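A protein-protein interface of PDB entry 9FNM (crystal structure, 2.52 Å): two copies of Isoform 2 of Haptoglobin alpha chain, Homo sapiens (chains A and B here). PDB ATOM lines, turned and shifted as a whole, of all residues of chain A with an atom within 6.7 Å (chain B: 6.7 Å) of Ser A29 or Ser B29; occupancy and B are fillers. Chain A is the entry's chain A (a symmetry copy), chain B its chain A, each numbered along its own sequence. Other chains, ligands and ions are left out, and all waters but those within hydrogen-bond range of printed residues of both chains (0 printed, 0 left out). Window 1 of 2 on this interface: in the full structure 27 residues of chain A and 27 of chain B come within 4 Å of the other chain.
The backbone NH of Glu B27 is in hydrogen-bond range of the backbone carbonyl oxygen of Arg A31 (3.2 Å).
The backbone NH of Ser B29 is in hydrogen-bond range of the backbone carbonyl oxygen of Ser A29.
The backbone NH of Glu A27 lies within hydrogen-bond range of the backbone carbonyl oxygen of Arg B31, 3.2 Å away.
Glu A27 touches Val B30.
O of Ser B29 touches CA of His A28 (3.95 Å).
His A28 touches Val B30 (NE2 to CG2, 3.9 Å).
O of Ser A29 touches CA of His B28, 3.95 Å away.
O of Glu B27 touches CA of Val A30 (3.8 Å).
His B28 touches Val A30.
Glu A27 touches Val B30, and with the chains exchanged Val A30 touches Glu B27.
Glu A27 touches Arg B31, and with the chains exchanged Arg A31 touches Glu B27.
His A28 touches Ser B29, and with the chains exchanged Ser A29 touches His B28.
Ser A29 touches its own counterpart, Ser B29.
10 positions are printed for both chains.
Of the 9 pairs that touch across the chains among the printed residues, 9 have their exchanged pair printed and touching as well.
The backbone carbonyl oxygen (O) of His B28 lies within hydrogen-bond range of the backbone NH (N) of Leu B50.
OG of Ser B29 sits at hydrogen-bond distance from OG1 of Thr B49.
N of Tyr B48 sits at hydrogen-bond distance from O of Val B30, 2.7 Å away.
The backbone carbonyl oxygen (O) of His A28 sits at hydrogen-bond distance from the backbone NH (N) of Leu A50 (2.9 Å).
The side-chain hydroxyl (OG1) of Thr A49 is in hydrogen-bond range of the side-chain hydroxyl (OG) of Ser A29.
N of Tyr A48 is in hydrogen-bond range of O of Val A30 (2.7 Å).
Ser A29 touches two residues of chain B.
Of chain A, only His A28 and Ser A29 come within 4 Å of Ser B29.
Of the printed residues of chain B, Glu A27 touches Val B30 (3.8 Å) and Arg B31 (3.2 Å).
Printed residues of chain B within 4 Å of Val A30: Glu B27 (3.8 Å) and His B28 (3.9 Å).
Of the printed residues of chain B, His A28 touches Ser B29 (3.95 Å) and Val B30 (3.9 Å).
Printed residues of chain A within 4 Å of His B28: Ser A29 and Val A30.
Of the printed residues of chain A, Val B30 touches Glu A27 (3.8 Å) and His A28 (3.9 Å).
Thr A49 touches none of the printed residues of chain B.
Trp A56 touches none of the printed residues of chain B.
The nearest residue of chain B that does not touch Ser A29 is Glu B27 (4.4 Å).
The nearest printed residue of chain A that does not touch Glu B27 is Ser A29 (4.4 Å).
Hydrophobic or aromatic side chains of chain B within 4 Å of the printed part of chain A: His B28 and Val B30.
Hydrophobic or aromatic side chains of chain A that line the printed part of chain B: His A28 and Val A30.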
ATOM      1  N   GLU A  27      -9.465   8.978   0.775  1.00  0.00           N
ATOM      2  CA  GLU A  27      -8.159   9.614   0.675  1.00  0.00           C
ATOM      3  C   GLU A  27      -8.235  10.647  -0.440  1.00  0.00           C
ATOM      4  O   GLU A  27      -8.727  10.353  -1.536  1.00  0.00           O
ATOM      5  CB  GLU A  27      -7.040   8.596   0.420  1.00  0.00           C
ATOM      6  CG  GLU A  27      -7.018   7.957  -0.959  1.00  0.00           C
ATOM      7  CD  GLU A  27      -5.645   7.419  -1.325  1.00  0.00           C
ATOM      8  OE1 GLU A  27      -4.840   7.154  -0.406  1.00  0.00           O
ATOM      9  OE2 GLU A  27      -5.371   7.271  -2.534  1.00  0.00           O
ATOM     10  N   HIS A  28      -7.795  11.865  -0.146  1.00  0.00           N
ATOM     11  CA  HIS A  28      -7.940  12.967  -1.082  1.00  0.00           C
ATOM     12  C   HIS A  28      -6.718  13.062  -1.983  1.00  0.00           C
ATOM     13  O   HIS A  28      -5.580  13.062  -1.502  1.00  0.00           O
ATOM     14  CB  HIS A  28      -8.160  14.283  -0.335  1.00  0.00           C
ATOM     15  CG  HIS A  28      -9.598  14.567  -0.024  1.00  0.00           C
ATOM     16  ND1 HIS A  28     -10.228  14.076   1.099  1.00  0.00           N
ATOM     17  CD2 HIS A  28     -10.530  15.284  -0.695  1.00  0.00           C
ATOM     18  CE1 HIS A  28     -11.486  14.481   1.107  1.00  0.00           C
ATOM     19  NE2 HIS A  28     -11.695  15.215   0.029  1.00  0.00           N
ATOM     20  N   SER A  29      -6.959  13.124  -3.288  1.00  0.00           N
ATOM     21  CA  SER A  29      -5.925  13.403  -4.270  1.00  0.00           C
ATOM     22  C   SER A  29      -6.211  14.745  -4.926  1.00  0.00           C
ATOM     23  O   SER A  29      -7.345  15.231  -4.930  1.00  0.00           O
ATOM     24  CB  SER A  29      -5.837  12.304  -5.338  1.00  0.00           C
ATOM     25  OG  SER A  29      -4.764  11.416  -5.071  1.00  0.00           O
ATOM     26  N   VAL A  30      -5.162  15.347  -5.475  1.00  0.00           N
ATOM     27  CA  VAL A  30      -5.290  16.611  -6.189  1.00  0.00           C
ATOM     28  C   VAL A  30      -4.325  16.589  -7.365  1.00  0.00           C
ATOM     29  O   VAL A  30      -3.219  16.045  -7.271  1.00  0.00           O
ATOM     30  CB  VAL A  30      -5.051  17.816  -5.249  1.00  0.00           C
ATOM     31  CG1 VAL A  30      -3.667  18.425  -5.444  1.00  0.00           C
ATOM     32  CG2 VAL A  30      -6.133  18.858  -5.447  1.00  0.00           C
ATOM     33  N   ARG A  31      -4.765  17.149  -8.490  1.00  0.00           N
ATOM     34  CA  ARG A  31      -3.976  17.194  -9.715  1.00  0.00           C
ATOM     35  C   ARG A  31      -3.847  18.642 -10.161  1.00  0.00           C
ATOM     36  O   ARG A  31      -4.857  19.319 -10.387  1.00  0.00           O
ATOM     37  CB  ARG A  31      -4.611  16.345 -10.818  1.00  0.00           C
ATOM     38  CG  ARG A  31      -3.905  16.455 -12.166  1.00  0.00           C
ATOM     39  CD  ARG A  31      -4.313  15.340 -13.124  1.00  0.00           C
ATOM     40  NE  ARG A  31      -3.568  15.403 -14.376  1.00  0.00           N
ATOM     41  CZ  ARG A  31      -4.062  15.847 -15.524  1.00  0.00           C
ATOM     42  NH1 ARG A  31      -5.320  16.247 -15.625  1.00  0.00           N
ATOM     43  NH2 ARG A  31      -3.278  15.888 -16.597  1.00  0.00           N
ATOM     44  N   VAL A  47       0.390  15.086  -9.547  1.00  0.00           N
ATOM     45  CA  VAL A  47      -0.618  14.516  -8.660  1.00  0.00           C
ATOM     46  C   VAL A  47      -0.080  14.521  -7.237  1.00  0.00           C
ATOM     47  O   VAL A  47       1.047  14.074  -6.987  1.00  0.00           O
ATOM     48  CB  VAL A  47      -1.009  13.094  -9.101  1.00  0.00           C
ATOM     49  CG1 VAL A  47      -1.967  12.467  -8.101  1.00  0.00           C
ATOM     50  CG2 VAL A  47      -1.636  13.129 -10.486  1.00  0.00           C
ATOM     51  N   TYR A  48      -0.883  15.029  -6.307  1.00  0.00           N
ATOM     52  CA  TYR A  48      -0.504  15.129  -4.905  1.00  0.00           C
ATOM     53  C   TYR A  48      -1.587  14.485  -4.053  1.00  0.00           C
ATOM     54  O   TYR A  48      -2.778  14.737  -4.265  1.00  0.00           O
ATOM     55  CB  TYR A  48      -0.290  16.591  -4.495  1.00  0.00           C
ATOM     56  CG  TYR A  48       0.929  17.227  -5.130  1.00  0.00           C
ATOM     57  CD1 TYR A  48       0.922  17.612  -6.464  1.00  0.00           C
ATOM     58  CD2 TYR A  48       2.086  17.439  -4.395  1.00  0.00           C
ATOM     59  CE1 TYR A  48       2.033  18.186  -7.049  1.00  0.00           C
ATOM     60  CE2 TYR A  48       3.203  18.018  -4.970  1.00  0.00           C
ATOM     61  CZ  TYR A  48       3.171  18.387  -6.299  1.00  0.00           C
ATOM     62  OH  TYR A  48       4.277  18.961  -6.880  1.00  0.00           O
ATOM     63  N   THR A  49      -1.175  13.652  -3.101  1.00  0.00           N
ATOM     64  CA  THR A  49      -2.090  12.935  -2.225  1.00  0.00           C
ATOM     65  C   THR A  49      -1.927  13.424  -0.791  1.00  0.00           C
ATOM     66  O   THR A  49      -0.805  13.586  -0.303  1.00  0.00           O
ATOM     67  CB  THR A  49      -1.848  11.422  -2.293  1.00  0.00           C
ATOM     68  OG1 THR A  49      -1.973  10.977  -3.650  1.00  0.00           O
ATOM     69  CG2 THR A  49      -2.859  10.674  -1.427  1.00  0.00           C
ATOM     70  N   LEU A  50      -3.054  13.648  -0.117  1.00  0.00           N
ATOM     71  CA  LEU A  50      -3.056  14.134   1.256  1.00  0.00           C
ATOM     72  C   LEU A  50      -2.812  12.973   2.213  1.00  0.00           C
ATOM     73  O   LEU A  50      -3.556  11.985   2.198  1.00  0.00           O
ATOM     74  CB  LEU A  50      -4.388  14.816   1.559  1.00  0.00           C
ATOM     75  CG  LEU A  50      -4.667  15.275   2.988  1.00  0.00           C
ATOM     76  CD1 LEU A  50      -3.789  16.457   3.359  1.00  0.00           C
ATOM     77  CD2 LEU A  50      -6.135  15.627   3.138  1.00  0.00           C
ATOM     78  N   TRP A  56       0.092  17.445   1.425  1.00  0.00           N
ATOM     79  CA  TRP A  56      -0.162  16.964   0.071  1.00  0.00           C
ATOM     80  C   TRP A  56       1.165  16.510  -0.524  1.00  0.00           C
ATOM     81  O   TRP A  56       2.040  17.333  -0.809  1.00  0.00           O
ATOM     82  CB  TRP A  56      -0.810  18.057  -0.772  1.00  0.00           C
ATOM     83  CG  TRP A  56      -2.126  18.515  -0.227  1.00  0.00           C
ATOM     84  CD1 TRP A  56      -2.335  19.455   0.740  1.00  0.00           C
ATOM     85  CD2 TRP A  56      -3.419  18.042  -0.614  1.00  0.00           C
ATOM     86  NE1 TRP A  56      -3.681  19.597   0.977  1.00  0.00           N
ATOM     87  CE2 TRP A  56      -4.368  18.741   0.157  1.00  0.00           C
ATOM     88  CE3 TRP A  56      -3.866  17.096  -1.540  1.00  0.00           C
ATOM     89  CZ2 TRP A  56      -5.738  18.524   0.030  1.00  0.00           C
ATOM     90  CZ3 TRP A  56      -5.225  16.882  -1.665  1.00  0.00           C
ATOM     91  CH2 TRP A  56      -6.146  17.592  -0.885  1.00  0.00           C
ATOM     92  N   GLU B  27      -7.908  19.991  -9.909  1.00  0.00           N
ATOM     93  CA  GLU B  27      -9.094  19.151 -10.002  1.00  0.00           C
ATOM     94  C   GLU B  27      -9.031  18.139  -8.867  1.00  0.00           C
ATOM     95  O   GLU B  27      -7.991  17.505  -8.647  1.00  0.00           O
ATOM     96  CB  GLU B  27      -9.203  18.455 -11.365  1.00  0.00           C
ATOM     97  CG  GLU B  27      -8.196  17.350 -11.636  1.00  0.00           C
ATOM     98  CD  GLU B  27      -8.676  16.376 -12.697  1.00  0.00           C
ATOM     99  OE1 GLU B  27      -9.549  16.756 -13.509  1.00  0.00           O
ATOM    100  OE2 GLU B  27      -8.187  15.227 -12.714  1.00  0.00           O
ATOM    101  N   HIS B  28     -10.121  18.025  -8.118  1.00  0.00           N
ATOM    102  CA  HIS B  28     -10.136  17.193  -6.925  1.00  0.00           C
ATOM    103  C   HIS B  28     -10.581  15.779  -7.271  1.00  0.00           C
ATOM    104  O   HIS B  28     -11.605  15.586  -7.934  1.00  0.00           O
ATOM    105  CB  HIS B  28     -11.049  17.797  -5.858  1.00  0.00           C
ATOM    106  CG  HIS B  28     -10.362  18.787  -4.967  1.00  0.00           C
ATOM    107  ND1 HIS B  28     -10.227  20.119  -5.296  1.00  0.00           N
ATOM    108  CD2 HIS B  28      -9.763  18.634  -3.762  1.00  0.00           C
ATOM    109  CE1 HIS B  28      -9.577  20.744  -4.330  1.00  0.00           C
ATOM    110  NE2 HIS B  28      -9.284  19.865  -3.388  1.00  0.00           N
ATOM    111  N   SER B  29      -9.798  14.800  -6.833  1.00  0.00           N
ATOM    112  CA  SER B  29     -10.169  13.397  -6.913  1.00  0.00           C
ATOM    113  C   SER B  29     -10.352  12.850  -5.506  1.00  0.00           C
ATOM    114  O   SER B  29      -9.824  13.392  -4.531  1.00  0.00           O
ATOM    115  CB  SER B  29      -9.120  12.568  -7.667  1.00  0.00           C
ATOM    116  OG  SER B  29      -9.525  12.323  -9.004  1.00  0.00           O
ATOM    117  N   VAL B  30     -11.119  11.770  -5.408  1.00  0.00           N
ATOM    118  CA  VAL B  30     -11.342  11.099  -4.134  1.00  0.00           C
ATOM    119  C   VAL B  30     -11.410   9.602  -4.393  1.00  0.00           C
ATOM    120  O   VAL B  30     -11.933   9.158  -5.421  1.00  0.00           O
ATOM    121  CB  VAL B  30     -12.609  11.637  -3.427  1.00  0.00           C
ATOM    122  CG1 VAL B  30     -13.786  10.679  -3.563  1.00  0.00           C
ATOM    123  CG2 VAL B  30     -12.312  11.928  -1.970  1.00  0.00           C
ATOM    124  N   ARG B  31     -10.843   8.825  -3.473  1.00  0.00           N
ATOM    125  CA  ARG B  31     -10.801   7.372  -3.579  1.00  0.00           C
ATOM    126  C   ARG B  31     -11.431   6.772  -2.331  1.00  0.00           C
ATOM    127  O   ARG B  31     -10.978   7.040  -1.212  1.00  0.00           O
ATOM    128  CB  ARG B  31      -9.367   6.867  -3.756  1.00  0.00           C
ATOM    129  CG  ARG B  31      -9.241   5.346  -3.739  1.00  0.00           C
ATOM    130  CD  ARG B  31      -7.896   4.873  -4.283  1.00  0.00           C
ATOM    131  NE  ARG B  31      -7.820   3.418  -4.346  1.00  0.00           N
ATOM    132  CZ  ARG B  31      -7.142   2.663  -3.492  1.00  0.00           C
ATOM    133  NH1 ARG B  31      -6.436   3.196  -2.508  1.00  0.00           N
ATOM    134  NH2 ARG B  31      -7.171   1.340  -3.630  1.00  0.00           N
ATOM    135  N   VAL B  47     -12.785   5.441  -7.563  1.00  0.00           N
ATOM    136  CA  VAL B  47     -12.230   6.781  -7.723  1.00  0.00           C
ATOM    137  C   VAL B  47     -13.312   7.697  -8.275  1.00  0.00           C
ATOM    138  O   VAL B  47     -13.977   7.363  -9.263  1.00  0.00           O
ATOM    139  CB  VAL B  47     -10.993   6.768  -8.637  1.00  0.00           C
ATOM    140  CG1 VAL B  47     -10.500   8.183  -8.893  1.00  0.00           C
ATOM    141  CG2 VAL B  47      -9.890   5.926  -8.015  1.00  0.00           C
ATOM    142  N   TYR B  48     -13.488   8.851  -7.636  1.00  0.00           N
ATOM    143  CA  TYR B  48     -14.500   9.822  -8.025  1.00  0.00           C
ATOM    144  C   TYR B  48     -13.837  11.180  -8.203  1.00  0.00           C
ATOM    145  O   TYR B  48     -13.043  11.601  -7.354  1.00  0.00           O
ATOM    146  CB  TYR B  48     -15.622   9.898  -6.982  1.00  0.00           C
ATOM    147  CG  TYR B  48     -16.480   8.653  -6.923  1.00  0.00           C
ATOM    148  CD1 TYR B  48     -16.015   7.490  -6.324  1.00  0.00           C
ATOM    149  CD2 TYR B  48     -17.755   8.641  -7.469  1.00  0.00           C
ATOM    150  CE1 TYR B  48     -16.793   6.349  -6.273  1.00  0.00           C
ATOM    151  CE2 TYR B  48     -18.544   7.506  -7.420  1.00  0.00           C
ATOM    152  CZ  TYR B  48     -18.056   6.362  -6.822  1.00  0.00           C
ATOM    153  OH  TYR B  48     -18.831   5.228  -6.770  1.00  0.00           O
ATOM    154  N   THR B  49     -14.156  11.855  -9.303  1.00  0.00           N
ATOM    155  CA  THR B  49     -13.585  13.153  -9.631  1.00  0.00           C
ATOM    156  C   THR B  49     -14.668  14.225  -9.591  1.00  0.00           C
ATOM    157  O   THR B  49     -15.770  14.028 -10.111  1.00  0.00           O
ATOM    158  CB  THR B  49     -12.921  13.131 -11.014  1.00  0.00           C
ATOM    159  OG1 THR B  49     -11.926  12.099 -11.051  1.00  0.00           O
ATOM    160  CG2 THR B  49     -12.260  14.473 -11.317  1.00  0.00           C
ATOM    161  N   LEU B  50     -14.343  15.362  -8.979  1.00  0.00           N
ATOM    162  CA  LEU B  50     -15.281  16.469  -8.846  1.00  0.00           C
ATOM    163  C   LEU B  50     -15.313  17.272 -10.141  1.00  0.00           C
ATOM    164  O   LEU B  50     -14.273  17.758 -10.601  1.00  0.00           O
ATOM    165  CB  LEU B  50     -14.873  17.352  -7.671  1.00  0.00           C
ATOM    166  CG  LEU B  50     -15.633  18.655  -7.435  1.00  0.00           C
ATOM    167  CD1 LEU B  50     -17.045  18.379  -6.950  1.00  0.00           C
ATOM    168  CD2 LEU B  50     -14.881  19.516  -6.438  1.00  0.00           C
ATOM    169  N   TRP B  56     -19.278  14.599  -7.654  1.00  0.00           N
ATOM    170  CA  TRP B  56     -18.177  13.642  -7.659  1.00  0.00           C
ATOM    171  C   TRP B  56     -18.557  12.490  -8.581  1.00  0.00           C
ATOM    172  O   TRP B  56     -19.452  11.700  -8.263  1.00  0.00           O
ATOM    173  CB  TRP B  56     -17.886  13.154  -6.242  1.00  0.00           C
ATOM    174  CG  TRP B  56     -17.490  14.258  -5.313  1.00  0.00           C
ATOM    175  CD1 TRP B  56     -18.323  15.083  -4.613  1.00  0.00           C
ATOM    176  CD2 TRP B  56     -16.158  14.663  -4.990  1.00  0.00           C
ATOM    177  NE1 TRP B  56     -17.587  15.976  -3.871  1.00  0.00           N
ATOM    178  CE2 TRP B  56     -16.255  15.737  -4.084  1.00  0.00           C
ATOM    179  CE3 TRP B  56     -14.891  14.219  -5.377  1.00  0.00           C
ATOM    180  CZ2 TRP B  56     -15.132  16.375  -3.561  1.00  0.00           C
ATOM    181  CZ3 TRP B  56     -13.779  14.852  -4.857  1.00  0.00           C
ATOM    182  CH2 TRP B  56     -13.906  15.918  -3.958  1.00  0.00           C
